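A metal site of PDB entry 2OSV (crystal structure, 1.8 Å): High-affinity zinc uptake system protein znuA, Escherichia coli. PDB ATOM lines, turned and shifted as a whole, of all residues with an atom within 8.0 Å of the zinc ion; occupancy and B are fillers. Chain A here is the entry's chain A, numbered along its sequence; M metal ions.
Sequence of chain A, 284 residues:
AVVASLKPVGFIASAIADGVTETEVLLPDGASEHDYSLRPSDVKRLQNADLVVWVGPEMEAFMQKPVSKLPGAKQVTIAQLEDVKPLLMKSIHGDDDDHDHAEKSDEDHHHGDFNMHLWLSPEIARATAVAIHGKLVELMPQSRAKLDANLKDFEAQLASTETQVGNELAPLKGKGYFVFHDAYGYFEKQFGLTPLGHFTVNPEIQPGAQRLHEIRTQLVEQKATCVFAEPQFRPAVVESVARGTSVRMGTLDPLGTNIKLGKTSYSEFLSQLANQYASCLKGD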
ATOM      1  N   LEU A   6       5.034  29.954 -23.622  1.00  0.00           N
ATOM      2  CA  LEU A   6       4.992  28.816 -22.693  1.00  0.00           C
ATOM      3  C   LEU A   6       3.540  28.433 -22.457  1.00  0.00           C
ATOM      4  O   LEU A   6       2.650  29.282 -22.498  1.00  0.00           O
ATOM      5  CB  LEU A   6       5.614  29.226 -21.340  1.00  0.00           C
ATOM      6  CG  LEU A   6       7.011  29.861 -21.347  1.00  0.00           C
ATOM      7  CD1 LEU A   6       7.360  30.326 -19.953  1.00  0.00           C
ATOM      8  CD2 LEU A   6       8.092  28.916 -21.897  1.00  0.00           C
ATOM      9  N   SER A  32      11.572  22.309 -21.244  1.00  0.00           N
ATOM     10  CA  SER A  32      11.736  23.297 -20.156  1.00  0.00           C
ATOM     11  C   SER A  32      11.915  24.709 -20.685  1.00  0.00           C
ATOM     12  O   SER A  32      12.587  24.920 -21.694  1.00  0.00           O
ATOM     13  CB  SER A  32      12.936  22.919 -19.302  1.00  0.00           C
ATOM     14  OG  SER A  32      13.220  23.940 -18.361  1.00  0.00           O
ATOM     15  N   GLU A  33      11.356  25.697 -19.971  1.00  0.00           N
ATOM     16  CA  GLU A  33      11.585  27.116 -20.284  1.00  0.00           C
ATOM     17  C   GLU A  33      13.082  27.473 -20.286  1.00  0.00           C
ATOM     18  O   GLU A  33      13.468  28.503 -20.835  1.00  0.00           O
ATOM     19  CB  GLU A  33      10.765  28.040 -19.344  1.00  0.00           C
ATOM     20  CG  GLU A  33      11.207  28.058 -17.841  1.00  0.00           C
ATOM     21  CD  GLU A  33      10.573  26.964 -16.974  1.00  0.00           C
ATOM     22  OE1 GLU A  33       9.992  26.018 -17.531  1.00  0.00           O
ATOM     23  OE2 GLU A  33      10.676  27.050 -15.708  1.00  0.00           O
ATOM     24  N   HIS A  34      13.907  26.622 -19.686  1.00  0.00           N
ATOM     25  CA  HIS A  34      15.341  26.913 -19.520  1.00  0.00           C
ATOM     26  C   HIS A  34      16.207  26.310 -20.601  1.00  0.00           C
ATOM     27  O   HIS A  34      17.442  26.433 -20.581  1.00  0.00           O
ATOM     28  CB  HIS A  34      15.796  26.436 -18.151  1.00  0.00           C
ATOM     29  CG  HIS A  34      15.090  27.144 -17.041  1.00  0.00           C
ATOM     30  ND1 HIS A  34      15.371  28.454 -16.706  1.00  0.00           N
ATOM     31  CD2 HIS A  34      14.058  26.760 -16.254  1.00  0.00           C
ATOM     32  CE1 HIS A  34      14.553  28.839 -15.731  1.00  0.00           C
ATOM     33  NE2 HIS A  34      13.751  27.821 -15.449  1.00  0.00           N
ATOM     34  N   MET A  59      13.747  35.694 -19.449  1.00  0.00           N
ATOM     35  CA  MET A  59      13.162  34.375 -19.309  1.00  0.00           C
ATOM     36  C   MET A  59      13.437  33.603 -20.619  1.00  0.00           C
ATOM     37  O   MET A  59      14.468  32.900 -20.697  1.00  0.00           O
ATOM     38  CB  MET A  59      11.670  34.488 -18.932  1.00  0.00           C
ATOM     39  CG  MET A  59      10.915  33.151 -18.718  1.00  0.00           C
ATOM     40  SD  MET A  59      11.677  31.930 -17.572  1.00  0.00           S
ATOM     41  CE  MET A  59      11.692  32.645 -16.045  1.00  0.00           C
ATOM     42  N   ASN A 115      12.802  37.359 -10.104  1.00  0.00           N
ATOM     43  CA  ASN A 115      12.180  36.089 -10.448  1.00  0.00           C
ATOM     44  C   ASN A 115      11.318  36.293 -11.681  1.00  0.00           C
ATOM     45  O   ASN A 115      10.400  37.136 -11.670  1.00  0.00           O
ATOM     46  CB  ASN A 115      11.263  35.701  -9.294  1.00  0.00           C
ATOM     47  CG  ASN A 115      10.739  34.289  -9.412  1.00  0.00           C
ATOM     48  OD1 ASN A 115      10.674  33.710 -10.502  1.00  0.00           O
ATOM     49  ND2 ASN A 115      10.361  33.731  -8.255  1.00  0.00           N
ATOM     50  N   MET A 116      11.601  35.527 -12.739  1.00  0.00           N
ATOM     51  CA  MET A 116      10.823  35.658 -13.975  1.00  0.00           C
ATOM     52  C   MET A 116       9.760  34.579 -14.197  1.00  0.00           C
ATOM     53  O   MET A 116       9.205  34.477 -15.292  1.00  0.00           O
ATOM     54  CB  MET A 116      11.771  35.752 -15.185  1.00  0.00           C
ATOM     55  CG  MET A 116      12.475  37.086 -15.320  1.00  0.00           C
ATOM     56  SD  MET A 116      11.376  38.440 -15.825  1.00  0.00           S
ATOM     57  CE  MET A 116      12.063  39.798 -14.892  1.00  0.00           C
ATOM     58  N   HIS A 117       9.444  33.778 -13.167  1.00  0.00           N
ATOM     59  CA  HIS A 117       8.407  32.744 -13.330  1.00  0.00           C
ATOM     60  C   HIS A 117       7.029  33.351 -13.089  1.00  0.00           C
ATOM     61  O   HIS A 117       6.283  32.970 -12.157  1.00  0.00           O
ATOM     62  CB  HIS A 117       8.679  31.571 -12.404  1.00  0.00           C
ATOM     63  CG  HIS A 117       9.896  30.790 -12.790  1.00  0.00           C
ATOM     64  ND1 HIS A 117      11.169  31.183 -12.434  1.00  0.00           N
ATOM     65  CD2 HIS A 117      10.031  29.685 -13.547  1.00  0.00           C
ATOM     66  CE1 HIS A 117      12.039  30.310 -12.933  1.00  0.00           C
ATOM     67  NE2 HIS A 117      11.366  29.388 -13.604  1.00  0.00           N
ATOM     68  N   TRP A 119       4.158  33.514 -14.652  1.00  0.00           N
ATOM     69  CA  TRP A 119       2.847  32.917 -14.984  1.00  0.00           C
ATOM     70  C   TRP A 119       2.218  32.201 -13.778  1.00  0.00           C
ATOM     71  O   TRP A 119       1.057  31.744 -13.872  1.00  0.00           O
ATOM     72  CB  TRP A 119       2.958  31.964 -16.171  1.00  0.00           C
ATOM     73  CG  TRP A 119       3.945  30.839 -15.934  1.00  0.00           C
ATOM     74  CD1 TRP A 119       3.658  29.589 -15.420  1.00  0.00           C
ATOM     75  CD2 TRP A 119       5.349  30.862 -16.180  1.00  0.00           C
ATOM     76  NE1 TRP A 119       4.817  28.849 -15.330  1.00  0.00           N
ATOM     77  CE2 TRP A 119       5.867  29.599 -15.811  1.00  0.00           C
ATOM     78  CE3 TRP A 119       6.237  31.835 -16.692  1.00  0.00           C
ATOM     79  CZ2 TRP A 119       7.238  29.272 -15.916  1.00  0.00           C
ATOM     80  CZ3 TRP A 119       7.609  31.512 -16.819  1.00  0.00           C
ATOM     81  CH2 TRP A 119       8.092  30.240 -16.417  1.00  0.00           C
ATOM     82  N   HIS A 181      13.325  22.811  -9.042  1.00  0.00           N
ATOM     83  CA  HIS A 181      13.901  24.104  -9.385  1.00  0.00           C
ATOM     84  C   HIS A 181      13.049  25.273  -8.920  1.00  0.00           C
ATOM     85  O   HIS A 181      11.854  25.109  -8.618  1.00  0.00           O
ATOM     86  CB  HIS A 181      14.348  24.187 -10.865  1.00  0.00           C
ATOM     87  CG  HIS A 181      13.352  24.796 -11.808  1.00  0.00           C
ATOM     88  ND1 HIS A 181      12.300  24.080 -12.346  1.00  0.00           N
ATOM     89  CD2 HIS A 181      13.299  26.021 -12.374  1.00  0.00           C
ATOM     90  CE1 HIS A 181      11.646  24.847 -13.206  1.00  0.00           C
ATOM     91  NE2 HIS A 181      12.223  26.035 -13.226  1.00  0.00           N
ATOM     92  N   ASP A 182      13.701  26.436  -8.831  1.00  0.00           N
ATOM     93  CA  ASP A 182      13.113  27.623  -8.173  1.00  0.00           C
ATOM     94  C   ASP A 182      12.108  28.344  -9.089  1.00  0.00           C
ATOM     95  O   ASP A 182      12.389  29.425  -9.626  1.00  0.00           O
ATOM     96  CB  ASP A 182      14.260  28.548  -7.719  1.00  0.00           C
ATOM     97  CG  ASP A 182      13.777  29.732  -6.902  1.00  0.00           C
ATOM     98  OD1 ASP A 182      12.641  29.695  -6.395  1.00  0.00           O
ATOM     99  OD2 ASP A 182      14.553  30.703  -6.766  1.00  0.00           O
ATOM    100  N   ALA A 183      10.939  27.738  -9.261  1.00  0.00           N
ATOM    101  CA  ALA A 183       9.940  28.207 -10.222  1.00  0.00           C
ATOM    102  C   ALA A 183       8.666  28.739  -9.566  1.00  0.00           C
ATOM    103  O   ALA A 183       7.822  29.309 -10.263  1.00  0.00           O
ATOM    104  CB  ALA A 183       9.558  27.082 -11.180  1.00  0.00           C
ATOM    105  N   TYR A 184       8.523  28.535  -8.264  1.00  0.00           N
ATOM    106  CA  TYR A 184       7.199  28.597  -7.632  1.00  0.00           C
ATOM    107  C   TYR A 184       6.988  29.777  -6.717  1.00  0.00           C
ATOM    108  O   TYR A 184       5.906  29.919  -6.129  1.00  0.00           O
ATOM    109  CB  TYR A 184       6.881  27.263  -6.884  1.00  0.00           C
ATOM    110  CG  TYR A 184       7.147  26.061  -7.760  1.00  0.00           C
ATOM    111  CD1 TYR A 184       6.160  25.567  -8.608  1.00  0.00           C
ATOM    112  CD2 TYR A 184       8.410  25.446  -7.785  1.00  0.00           C
ATOM    113  CE1 TYR A 184       6.410  24.484  -9.457  1.00  0.00           C
ATOM    114  CE2 TYR A 184       8.671  24.361  -8.647  1.00  0.00           C
ATOM    115  CZ  TYR A 184       7.663  23.885  -9.471  1.00  0.00           C
ATOM    116  OH  TYR A 184       7.899  22.830 -10.320  1.00  0.00           O
ATOM    117  N   VAL A 201      18.533  26.276  -9.106  1.00  0.00           N
ATOM    118  CA  VAL A 201      17.893  27.484  -9.631  1.00  0.00           C
ATOM    119  C   VAL A 201      17.583  27.214 -11.100  1.00  0.00           C
ATOM    120  O   VAL A 201      16.419  27.275 -11.531  1.00  0.00           O
ATOM    121  CB  VAL A 201      18.763  28.730  -9.442  1.00  0.00           C
ATOM    122  CG1 VAL A 201      18.163  29.943 -10.158  1.00  0.00           C
ATOM    123  CG2 VAL A 201      18.921  29.032  -7.943  1.00  0.00           C
ATOM    124  N   ASN A 202      18.620  26.900 -11.867  1.00  0.00           N
ATOM    125  CA  ASN A 202      18.471  26.485 -13.266  1.00  0.00           C
ATOM    126  C   ASN A 202      18.529  24.951 -13.317  1.00  0.00           C
ATOM    127  O   ASN A 202      19.578  24.366 -12.976  1.00  0.00           O
ATOM    128  CB  ASN A 202      19.597  27.099 -14.097  1.00  0.00           C
ATOM    129  CG  ASN A 202      19.525  26.723 -15.567  1.00  0.00           C
ATOM    130  OD1 ASN A 202      18.794  25.810 -15.959  1.00  0.00           O
ATOM    131  ND2 ASN A 202      20.288  27.437 -16.390  1.00  0.00           N
ATOM    132  N   PRO A 203      17.431  24.289 -13.744  1.00  0.00           N
ATOM    133  CA  PRO A 203      17.408  22.827 -13.655  1.00  0.00           C
ATOM    134  C   PRO A 203      18.335  22.136 -14.666  1.00  0.00           C
ATOM    135  O   PRO A 203      18.491  20.918 -14.629  1.00  0.00           O
ATOM    136  CB  PRO A 203      15.936  22.471 -13.915  1.00  0.00           C
ATOM    137  CG  PRO A 203      15.417  23.636 -14.754  1.00  0.00           C
ATOM    138  CD  PRO A 203      16.177  24.844 -14.304  1.00  0.00           C
ATOM    139  N   GLU A 230       9.793  17.081 -11.001  1.00  0.00           N
ATOM    140  CA  GLU A 230       9.084  17.796 -12.089  1.00  0.00           C
ATOM    141  C   GLU A 230       9.097  16.925 -13.346  1.00  0.00           C
ATOM    142  O   GLU A 230      10.073  16.230 -13.588  1.00  0.00           O
ATOM    143  CB  GLU A 230       9.749  19.155 -12.386  1.00  0.00           C
ATOM    144  CG  GLU A 230       9.697  20.077 -11.169  1.00  0.00           C
ATOM    145  CD  GLU A 230      10.567  21.314 -11.254  1.00  0.00           C
ATOM    146  OE1 GLU A 230      11.290  21.489 -12.261  1.00  0.00           O
ATOM    147  OE2 GLU A 230      10.522  22.104 -10.271  1.00  0.00           O
ATOM    148  N   PHE A 233      12.067  16.795 -15.973  1.00  0.00           N
ATOM    149  CA  PHE A 233      13.387  16.304 -15.549  1.00  0.00           C
ATOM    150  C   PHE A 233      13.336  14.931 -14.916  1.00  0.00           C
ATOM    151  O   PHE A 233      12.398  14.626 -14.172  1.00  0.00           O
ATOM    152  CB  PHE A 233      14.046  17.333 -14.616  1.00  0.00           C
ATOM    153  CG  PHE A 233      14.257  18.642 -15.296  1.00  0.00           C
ATOM    154  CD1 PHE A 233      15.349  18.815 -16.150  1.00  0.00           C
ATOM    155  CD2 PHE A 233      13.315  19.658 -15.191  1.00  0.00           C
ATOM    156  CE1 PHE A 233      15.520  20.005 -16.852  1.00  0.00           C
ATOM    157  CE2 PHE A 233      13.478  20.855 -15.891  1.00  0.00           C
ATOM    158  CZ  PHE A 233      14.586  21.026 -16.718  1.00  0.00           C
ATOM    159  N   PRO A 254       5.361  23.011 -13.360  1.00  0.00           N
ATOM    160  CA  PRO A 254       5.162  24.475 -13.478  1.00  0.00           C
ATOM    161  C   PRO A 254       4.679  24.913 -14.863  1.00  0.00           C
ATOM    162  O   PRO A 254       4.458  26.107 -15.088  1.00  0.00           O
ATOM    163  CB  PRO A 254       6.556  25.030 -13.185  1.00  0.00           C
ATOM    164  CG  PRO A 254       7.530  23.935 -13.773  1.00  0.00           C
ATOM    165  CD  PRO A 254       6.793  22.624 -13.400  1.00  0.00           C
ATOM    166  N   LEU A 255       4.536  23.966 -15.785  1.00  0.00           N
ATOM    167  CA  LEU A 255       4.127  24.265 -17.149  1.00  0.00           C
ATOM    168  C   LEU A 255       2.779  23.642 -17.550  1.00  0.00           C
ATOM    169  O   LEU A 255       2.351  23.761 -18.699  1.00  0.00           O
ATOM    170  CB  LEU A 255       5.240  23.912 -18.155  1.00  0.00           C
ATOM    171  CG  LEU A 255       6.557  24.688 -18.002  1.00  0.00           C
ATOM    172  CD1 LEU A 255       7.616  24.124 -18.936  1.00  0.00           C
ATOM    173  CD2 LEU A 255       6.324  26.169 -18.313  1.00  0.00           C
HETATM  174 ZN    ZN M   1      11.954  27.652 -14.510  1.00  0.00          ZN
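The backbone NH (N) of His 117 lies within hydrogen-bond range of the side-chain amide oxygen (OD1) of Asn 115.
The backbone NH (N) of His 34 sits close to the side-chain hydroxyl (OG) of Ser 32 (3.1 Å).
OE1 of Glu 230 lies within hydrogen-bond range of ND1 of His 181 (2.8 Å).
Of the 20 residues printed, 4 come within 4 Å of the zinc ion.
The nearest printed residue that does not touch the zinc ion is Ala 183 (4.1 Å).
The zinc ion is bound by the side-chain carboxylate (OE2) of Glu 33 (1.9 Å), a ring nitrogen (NE2) of His 34 (2.0 Å), a ring nitrogen (NE2) of His 117 (2.0 Å) and a ring nitrogen (NE2) of His 181 (2.1 Å).
The zinc ion has four donor atoms within binding distance.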
